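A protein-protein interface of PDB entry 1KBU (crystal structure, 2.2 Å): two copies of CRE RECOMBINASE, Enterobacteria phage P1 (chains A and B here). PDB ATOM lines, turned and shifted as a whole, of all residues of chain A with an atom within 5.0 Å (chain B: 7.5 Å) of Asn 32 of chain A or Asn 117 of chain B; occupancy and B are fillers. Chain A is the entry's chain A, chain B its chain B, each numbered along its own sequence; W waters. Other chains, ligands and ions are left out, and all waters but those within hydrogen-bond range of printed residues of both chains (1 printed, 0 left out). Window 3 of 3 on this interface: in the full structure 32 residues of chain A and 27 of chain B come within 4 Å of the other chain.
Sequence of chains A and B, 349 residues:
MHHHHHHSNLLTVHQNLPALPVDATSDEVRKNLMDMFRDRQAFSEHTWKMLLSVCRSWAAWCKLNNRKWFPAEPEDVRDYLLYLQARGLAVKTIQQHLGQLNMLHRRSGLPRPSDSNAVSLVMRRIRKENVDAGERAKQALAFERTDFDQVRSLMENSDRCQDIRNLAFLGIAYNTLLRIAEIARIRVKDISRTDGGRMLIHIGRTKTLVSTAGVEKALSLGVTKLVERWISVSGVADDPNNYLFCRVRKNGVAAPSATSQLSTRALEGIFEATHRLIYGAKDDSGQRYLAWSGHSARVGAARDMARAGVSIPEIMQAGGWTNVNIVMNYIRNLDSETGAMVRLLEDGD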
ATOM      1  N   GLU A  28      20.681  28.839  15.892  1.00  0.00           N
ATOM      2  CA  GLU A  28      20.988  28.893  14.470  1.00  0.00           C
ATOM      3  C   GLU A  28      21.438  27.506  14.044  1.00  0.00           C
ATOM      4  O   GLU A  28      21.012  26.980  13.016  1.00  0.00           O
ATOM      5  CB  GLU A  28      22.141  29.856  14.231  1.00  0.00           C
ATOM      6  CG  GLU A  28      21.749  31.109  13.488  1.00  0.00           C
ATOM      7  CD  GLU A  28      22.478  32.307  14.033  1.00  0.00           C
ATOM      8  OE1 GLU A  28      22.510  32.416  15.271  1.00  0.00           O
ATOM      9  OE2 GLU A  28      23.019  33.124  13.260  1.00  0.00           O
ATOM     10  N   VAL A  29      22.319  26.935  14.859  1.00  0.00           N
ATOM     11  CA  VAL A  29      22.850  25.598  14.629  1.00  0.00           C
ATOM     12  C   VAL A  29      21.726  24.563  14.563  1.00  0.00           C
ATOM     13  O   VAL A  29      21.654  23.768  13.627  1.00  0.00           O
ATOM     14  CB  VAL A  29      23.910  25.220  15.682  1.00  0.00           C
ATOM     15  CG1 VAL A  29      24.421  23.800  15.453  1.00  0.00           C
ATOM     16  CG2 VAL A  29      25.050  26.240  15.655  1.00  0.00           C
ATOM     17  N   ARG A  30      20.831  24.591  15.541  1.00  0.00           N
ATOM     18  CA  ARG A  30      19.706  23.659  15.579  1.00  0.00           C
ATOM     19  C   ARG A  30      18.836  23.812  14.334  1.00  0.00           C
ATOM     20  O   ARG A  30      18.305  22.828  13.823  1.00  0.00           O
ATOM     21  CB  ARG A  30      18.896  23.866  16.863  1.00  0.00           C
ATOM     22  CG  ARG A  30      17.646  23.004  17.021  1.00  0.00           C
ATOM     23  CD  ARG A  30      16.775  23.490  18.183  1.00  0.00           C
ATOM     24  NE  ARG A  30      17.400  23.299  19.494  1.00  0.00           N
ATOM     25  CZ  ARG A  30      17.748  22.114  19.992  1.00  0.00           C
ATOM     26  NH1 ARG A  30      17.537  21.011  19.290  1.00  0.00           N
ATOM     27  NH2 ARG A  30      18.313  22.024  21.190  1.00  0.00           N
ATOM     28  N   LYS A  31      18.699  25.036  13.831  1.00  0.00           N
ATOM     29  CA  LYS A  31      17.930  25.288  12.609  1.00  0.00           C
ATOM     30  C   LYS A  31      18.706  24.702  11.406  1.00  0.00           C
ATOM     31  O   LYS A  31      18.140  24.058  10.516  1.00  0.00           O
ATOM     32  CB  LYS A  31      17.708  26.797  12.453  1.00  0.00           C
ATOM     33  CG  LYS A  31      17.249  27.242  11.066  1.00  0.00           C
ATOM     34  CD  LYS A  31      15.958  26.564  10.626  1.00  0.00           C
ATOM     35  CE  LYS A  31      15.257  27.404   9.569  1.00  0.00           C
ATOM     36  NZ  LYS A  31      15.734  27.156   8.186  1.00  0.00           N
ATOM     37  N   ASN A  32      20.014  24.950  11.380  1.00  0.00           N
ATOM     38  CA  ASN A  32      20.895  24.420  10.341  1.00  0.00           C
ATOM     39  C   ASN A  32      20.863  22.879  10.299  1.00  0.00           C
ATOM     40  O   ASN A  32      20.764  22.296   9.222  1.00  0.00           O
ATOM     41  CB  ASN A  32      22.327  24.895  10.572  1.00  0.00           C
ATOM     42  CG  ASN A  32      22.529  26.322  10.150  1.00  0.00           C
ATOM     43  OD1 ASN A  32      21.790  26.836   9.315  1.00  0.00           O
ATOM     44  ND2 ASN A  32      23.532  26.976  10.716  1.00  0.00           N
ATOM     45  N   LEU A  33      20.929  22.216  11.455  1.00  0.00           N
ATOM     46  CA  LEU A  33      20.881  20.755  11.505  1.00  0.00           C
ATOM     47  C   LEU A  33      19.531  20.182  11.063  1.00  0.00           C
ATOM     48  O   LEU A  33      19.496  19.140  10.413  1.00  0.00           O
ATOM     49  CB  LEU A  33      21.354  20.203  12.853  1.00  0.00           C
ATOM     50  CG  LEU A  33      22.770  20.643  13.266  1.00  0.00           C
ATOM     51  CD1 LEU A  33      23.115  20.286  14.709  1.00  0.00           C
ATOM     52  CD2 LEU A  33      23.870  20.185  12.315  1.00  0.00           C
ATOM     53  N   MET A  34      18.424  20.869  11.360  1.00  0.00           N
ATOM     54  CA  MET A  34      17.103  20.423  10.889  1.00  0.00           C
ATOM     55  C   MET A  34      17.019  20.624   9.351  1.00  0.00           C
ATOM     56  O   MET A  34      16.372  19.847   8.632  1.00  0.00           O
ATOM     57  CB  MET A  34      15.991  21.229  11.575  1.00  0.00           C
ATOM     58  CG  MET A  34      16.007  21.229  13.105  1.00  0.00           C
ATOM     59  SD  MET A  34      14.619  22.179  13.781  1.00  0.00           S
ATOM     60  CE  MET A  34      14.013  21.090  15.081  1.00  0.00           C
ATOM     61  N   ASP A  35      17.670  21.684   8.866  1.00  0.00           N
ATOM     62  CA  ASP A  35      17.717  21.990   7.436  1.00  0.00           C
ATOM     63  C   ASP A  35      18.380  20.770   6.780  1.00  0.00           C
ATOM     64  O   ASP A  35      17.878  20.243   5.787  1.00  0.00           O
ATOM     65  CB  ASP A  35      18.603  23.220   7.187  1.00  0.00           C
ATOM     66  CG  ASP A  35      17.859  24.540   7.278  1.00  0.00           C
ATOM     67  OD1 ASP A  35      16.632  24.551   7.499  1.00  0.00           O
ATOM     68  OD2 ASP A  35      18.530  25.582   7.134  1.00  0.00           O
ATOM     69  N   MET A  36      19.506  20.331   7.347  1.00  0.00           N
ATOM     70  CA  MET A  36      20.272  19.186   6.853  1.00  0.00           C
ATOM     71  C   MET A  36      19.442  17.910   6.796  1.00  0.00           C
ATOM     72  O   MET A  36      19.446  17.194   5.797  1.00  0.00           O
ATOM     73  CB  MET A  36      21.461  18.940   7.778  1.00  0.00           C
ATOM     74  CG  MET A  36      22.810  18.990   7.110  1.00  0.00           C
ATOM     75  SD  MET A  36      24.106  19.407   8.297  1.00  0.00           S
ATOM     76  CE  MET A  36      24.693  17.762   8.751  1.00  0.00           C
ATOM     77  N   ARG A 106      30.393  23.611   8.110  1.00  0.00           N
ATOM     78  CA  ARG A 106      30.050  24.572   7.067  1.00  0.00           C
ATOM     79  C   ARG A 106      28.536  24.632   6.901  1.00  0.00           C
ATOM     80  O   ARG A 106      27.948  25.698   6.728  1.00  0.00           O
ATOM     81  CB  ARG A 106      30.725  24.195   5.745  1.00  0.00           C
ATOM     82  CG  ARG A 106      30.636  25.267   4.668  1.00  0.00           C
ATOM     83  CD  ARG A 106      30.769  24.678   3.256  1.00  0.00           C
ATOM     84  NE  ARG A 106      31.981  23.868   3.089  1.00  0.00           N
ATOM     85  CZ  ARG A 106      32.011  22.616   2.642  1.00  0.00           C
ATOM     86  NH1 ARG A 106      30.892  21.976   2.319  1.00  0.00           N
ATOM     87  NH2 ARG A 106      33.175  21.979   2.555  1.00  0.00           N
ATOM     88  N   ARG A 107      27.920  23.458   6.989  1.00  0.00           N
ATOM     89  CA  ARG A 107      26.481  23.287   6.849  1.00  0.00           C
ATOM     90  C   ARG A 107      25.790  23.313   8.184  1.00  0.00           C
ATOM     91  O   ARG A 107      24.682  22.803   8.333  1.00  0.00           O
ATOM     92  CB  ARG A 107      26.199  21.924   6.266  1.00  0.00           C
ATOM     93  CG  ARG A 107      26.595  21.830   4.865  1.00  0.00           C
ATOM     94  CD  ARG A 107      25.428  22.278   4.092  1.00  0.00           C
ATOM     95  NE  ARG A 107      25.616  21.915   2.704  1.00  0.00           N
ATOM     96  CZ  ARG A 107      25.185  22.664   1.700  1.00  0.00           C
ATOM     97  NH1 ARG A 107      24.549  23.801   1.956  1.00  0.00           N
ATOM     98  NH2 ARG A 107      25.379  22.285   0.442  1.00  0.00           N
ATOM     99  N   SER A 108      26.441  23.881   9.182  1.00  0.00           N
ATOM    100  CA  SER A 108      25.778  24.009  10.463  1.00  0.00           C
ATOM    101  C   SER A 108      25.931  25.470  10.883  1.00  0.00           C
ATOM    102  O   SER A 108      25.264  25.937  11.800  1.00  0.00           O
ATOM    103  CB  SER A 108      26.210  22.981  11.513  1.00  0.00           C
ATOM    104  OG  SER A 108      27.448  23.343  12.095  1.00  0.00           O
ATOM    105  N   GLY A 109      26.803  26.204  10.198  1.00  0.00           N
ATOM    106  CA  GLY A 109      26.958  27.627  10.472  1.00  0.00           C
ATOM    107  C   GLY A 109      28.193  27.986  11.268  1.00  0.00           C
ATOM    108  O   GLY A 109      28.451  29.166  11.532  1.00  0.00           O
ATOM    109  N   PRO B  74      14.367  32.780   2.782  1.00  0.00           N
ATOM    110  CA  PRO B  74      14.854  31.477   2.358  1.00  0.00           C
ATOM    111  C   PRO B  74      13.769  30.415   2.398  1.00  0.00           C
ATOM    112  O   PRO B  74      13.490  29.780   1.387  1.00  0.00           O
ATOM    113  CB  PRO B  74      15.937  31.181   3.386  1.00  0.00           C
ATOM    114  CG  PRO B  74      16.540  32.529   3.608  1.00  0.00           C
ATOM    115  CD  PRO B  74      15.412  33.535   3.495  1.00  0.00           C
ATOM    116  N   GLU B  75      13.134  30.223   3.546  1.00  0.00           N
ATOM    117  CA  GLU B  75      12.089  29.207   3.640  1.00  0.00           C
ATOM    118  C   GLU B  75      11.003  29.346   2.578  1.00  0.00           C
ATOM    119  O   GLU B  75      10.381  28.360   2.176  1.00  0.00           O
ATOM    120  CB  GLU B  75      11.453  29.210   5.032  1.00  0.00           C
ATOM    121  CG  GLU B  75      12.397  28.798   6.146  1.00  0.00           C
ATOM    122  CD  GLU B  75      12.718  27.323   6.077  1.00  0.00           C
ATOM    123  OE1 GLU B  75      11.813  26.541   5.732  1.00  0.00           O
ATOM    124  OE2 GLU B  75      13.874  26.949   6.359  1.00  0.00           O
ATOM    125  N   ARG B  78      12.459  28.340  -0.777  1.00  0.00           N
ATOM    126  CA  ARG B  78      12.460  26.887  -0.795  1.00  0.00           C
ATOM    127  C   ARG B  78      11.120  26.270  -1.184  1.00  0.00           C
ATOM    128  O   ARG B  78      11.072  25.427  -2.072  1.00  0.00           O
ATOM    129  CB  ARG B  78      13.062  26.328   0.497  1.00  0.00           C
ATOM    130  CG  ARG B  78      12.827  24.856   0.735  1.00  0.00           C
ATOM    131  CD  ARG B  78      13.490  24.371   2.027  1.00  0.00           C
ATOM    132  NE  ARG B  78      13.429  22.913   2.068  1.00  0.00           N
ATOM    133  CZ  ARG B  78      12.304  22.225   2.218  1.00  0.00           C
ATOM    134  NH1 ARG B  78      11.167  22.872   2.439  1.00  0.00           N
ATOM    135  NH2 ARG B  78      12.334  20.895   2.180  1.00  0.00           N
ATOM    136  N   PRO B 113      19.311  34.134  -1.577  1.00  0.00           N
ATOM    137  CA  PRO B 113      18.569  32.984  -1.085  1.00  0.00           C
ATOM    138  C   PRO B 113      19.519  31.789  -1.007  1.00  0.00           C
ATOM    139  O   PRO B 113      19.618  31.121   0.026  1.00  0.00           O
ATOM    140  CB  PRO B 113      17.510  32.786  -2.162  1.00  0.00           C
ATOM    141  CG  PRO B 113      17.175  34.200  -2.551  1.00  0.00           C
ATOM    142  CD  PRO B 113      18.443  35.024  -2.378  1.00  0.00           C
ATOM    143  N   SER B 114      20.244  31.544  -2.092  1.00  0.00           N
ATOM    144  CA  SER B 114      21.177  30.431  -2.096  1.00  0.00           C
ATOM    145  C   SER B 114      22.172  30.468  -0.936  1.00  0.00           C
ATOM    146  O   SER B 114      22.872  29.492  -0.667  1.00  0.00           O
ATOM    147  CB  SER B 114      21.862  30.289  -3.448  1.00  0.00           C
ATOM    148  OG  SER B 114      21.028  29.543  -4.318  1.00  0.00           O
ATOM    149  N   ASP B 115      22.208  31.582  -0.216  1.00  0.00           N
ATOM    150  CA  ASP B 115      23.119  31.687   0.909  1.00  0.00           C
ATOM    151  C   ASP B 115      22.585  30.966   2.125  1.00  0.00           C
ATOM    152  O   ASP B 115      23.217  30.966   3.173  1.00  0.00           O
ATOM    153  CB  ASP B 115      23.372  33.143   1.246  1.00  0.00           C
ATOM    154  CG  ASP B 115      24.310  33.780   0.275  1.00  0.00           C
ATOM    155  OD1 ASP B 115      25.150  33.039  -0.269  1.00  0.00           O
ATOM    156  OD2 ASP B 115      24.214  35.006   0.063  1.00  0.00           O
ATOM    157  N   SER B 116      21.436  30.325   1.985  1.00  0.00           N
ATOM    158  CA  SER B 116      20.872  29.614   3.115  1.00  0.00           C
ATOM    159  C   SER B 116      20.761  28.124   2.844  1.00  0.00           C
ATOM    160  O   SER B 116      20.261  27.700   1.801  1.00  0.00           O
ATOM    161  CB  SER B 116      19.516  30.211   3.496  1.00  0.00           C
ATOM    162  OG  SER B 116      18.498  29.829   2.590  1.00  0.00           O
ATOM    163  N   ASN B 117      21.195  27.334   3.813  1.00  0.00           N
ATOM    164  CA  ASN B 117      21.109  25.895   3.692  1.00  0.00           C
ATOM    165  C   ASN B 117      19.764  25.521   3.118  1.00  0.00           C
ATOM    166  O   ASN B 117      19.680  24.675   2.242  1.00  0.00           O
ATOM    167  CB  ASN B 117      21.233  25.232   5.063  1.00  0.00           C
ATOM    168  CG  ASN B 117      22.654  25.096   5.503  1.00  0.00           C
ATOM    169  OD1 ASN B 117      23.563  25.179   4.688  1.00  0.00           O
ATOM    170  ND2 ASN B 117      22.863  24.865   6.790  1.00  0.00           N
ATOM    171  N   ALA B 118      18.680  26.085   3.646  1.00  0.00           N
ATOM    172  CA  ALA B 118      17.382  25.677   3.128  1.00  0.00           C
ATOM    173  C   ALA B 118      17.309  25.767   1.622  1.00  0.00           C
ATOM    174  O   ALA B 118      16.725  24.898   0.985  1.00  0.00           O
ATOM    175  CB  ALA B 118      16.237  26.454   3.755  1.00  0.00           C
ATOM    176  N   VAL B 119      17.844  26.841   1.052  1.00  0.00           N
ATOM    177  CA  VAL B 119      17.755  27.015  -0.390  1.00  0.00           C
ATOM    178  C   VAL B 119      18.837  26.231  -1.120  1.00  0.00           C
ATOM    179  O   VAL B 119      18.579  25.600  -2.142  1.00  0.00           O
ATOM    180  CB  VAL B 119      17.769  28.495  -0.768  1.00  0.00           C
ATOM    181  CG1 VAL B 119      17.524  28.648  -2.256  1.00  0.00           C
ATOM    182  CG2 VAL B 119      16.691  29.220   0.012  1.00  0.00           C
ATOM    183  N   SER B 120      20.043  26.273  -0.565  1.00  0.00           N
ATOM    184  CA  SER B 120      21.185  25.535  -1.085  1.00  0.00           C
ATOM    185  C   SER B 120      20.848  24.062  -1.250  1.00  0.00           C
ATOM    186  O   SER B 120      20.963  23.510  -2.338  1.00  0.00           O
ATOM    187  CB  SER B 120      22.338  25.636  -0.092  1.00  0.00           C
ATOM    188  OG  SER B 120      22.795  26.968  -0.078  1.00  0.00           O
ATOM    189  N   LEU B 121      20.447  23.423  -0.159  1.00  0.00           N
ATOM    190  CA  LEU B 121      20.142  22.002  -0.156  1.00  0.00           C
ATOM    191  C   LEU B 121      18.919  21.574  -0.933  1.00  0.00           C
ATOM    192  O   LEU B 121      18.872  20.442  -1.407  1.00  0.00           O
ATOM    193  CB  LEU B 121      20.008  21.476   1.273  1.00  0.00           C
ATOM    194  CG  LEU B 121      21.173  21.658   2.241  1.00  0.00           C
ATOM    195  CD1 LEU B 121      20.736  21.410   3.688  1.00  0.00           C
ATOM    196  CD2 LEU B 121      22.338  20.761   1.830  1.00  0.00           C
ATOM    197  N   VAL B 122      17.887  22.409  -0.998  1.00  0.00           N
ATOM    198  CA  VAL B 122      16.674  22.000  -1.708  1.00  0.00           C
ATOM    199  C   VAL B 122      17.013  21.986  -3.189  1.00  0.00           C
ATOM    200  O   VAL B 122      16.477  21.174  -3.939  1.00  0.00           O
ATOM    201  CB  VAL B 122      15.452  22.939  -1.451  1.00  0.00           C
ATOM    202  CG1 VAL B 122      15.468  24.145  -2.407  1.00  0.00           C
ATOM    203  CG2 VAL B 122      14.146  22.171  -1.627  1.00  0.00           C
ATOM    204  N   MET B 123      17.886  22.898  -3.609  1.00  0.00           N
ATOM    205  CA  MET B 123      18.266  22.968  -5.011  1.00  0.00           C
ATOM    206  C   MET B 123      18.934  21.625  -5.350  1.00  0.00           C
ATOM    207  O   MET B 123      18.471  20.901  -6.238  1.00  0.00           O
ATOM    208  CB  MET B 123      19.161  24.183  -5.285  1.00  0.00           C
ATOM    209  CG  MET B 123      19.132  24.693  -6.734  1.00  0.00           C
ATOM    210  SD  MET B 123      17.543  24.770  -7.638  1.00  0.00           S
ATOM    211  CE  MET B 123      17.421  23.169  -8.411  1.00  0.00           C
HETATM  212  O   HOH W   1      21.588  28.955   6.700  1.00  0.00           O
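The side-chain amide oxygen (OD1) of Asn 32 of chain A is in hydrogen-bond range of the side-chain amide nitrogen (ND2) of Asn 117 of chain B, at 3.4 Å.
O of Arg 107 of chain A lies within hydrogen-bond range of ND2 of Asn 117 of chain B (3.2 Å).
The side-chain carboxylate of Glu 75 of chain B is in salt-bridge range of the side-chain amino group of Lys 31 of chain A.
The side-chain hydroxyl (OG) of Ser 120 of chain B lies within hydrogen-bond range of the backbone carbonyl oxygen (O) of Ser 114 of chain B (2.6 Å).
NZ of Lys 31 of chain A lies within salt-bridge range of OD1 of Asp 35 of chain A, 2.8 Å away.
O of Glu 28 of chain A sits close to ND2 of Asn 32 of chain A.
The backbone carbonyl oxygen of Ser 116 of chain B is in hydrogen-bond range of the side-chain hydroxyl of Ser 120 of chain B (3.2 Å).
The side-chain amide nitrogen (ND2) of Asn 32 of chain A lies close to the backbone NH (N) of Gly 109 of chain A (3.4 Å).
Among the printed residues, merely in contact across the chains: Asp 35 of chain A with Asn 117 of chain B, Arg 107 of chain A with Leu 121 of chain B, Asp 35 of chain A with Ala 118 of chain B, Arg 107 of chain A with Ser 120 of chain B, Asp 35 of chain A with Leu 121 of chain B, Asp 35 of chain A with Glu 75 of chain B and Met 36 of chain A with Leu 121 of chain B.
Of the printed residues of chain B, Asn 32 of chain A touches Asn 117.
Asn 117 of chain B touches just these residues of chain A: Asn 32, Asp 35 and Arg 107.
Of the printed residues of chain A, Ala 118 of chain B touches Asp 35 (3.5 Å).
Printed residues of chain A within 4 Å of Glu 75 of chain B: Lys 31 (2.6 Å) and Asp 35 (3.8 Å).
Printed residues of chain A within 4 Å of Leu 121 of chain B: Asp 35 (3.7 Å), Met 36 (3.9 Å) and Arg 107 (3.4 Å).
Of the printed residues of chain B, Lys 31 of chain A touches Glu 75 (2.6 Å).
Printed residues of chain A within 4 Å of Ser 120 of chain B: Arg 107.
The nearest residue of chain A that does not touch Asn 117 of chain B is Ser 108 of chain A (4.4 Å).
The nearest printed residue of chain A that does not touch Glu 75 of chain B is Met 34 of chain A (7.7 Å).
Along chain A the printed residues that touch a printed residue of chain B span positions 31 to 107.
Among the printed residues, 10 pairs touch across the chains.
No position is printed for both chains.
Of the 10 pairs that touch across the chains among the printed residues, none has its exchanged pair printed and touching as well.
Water W1 lies within hydrogen-bond range of N of Asn 117 of chain B (3.3 Å) and OD1 of Asn 32 of chain A (3.4 Å).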
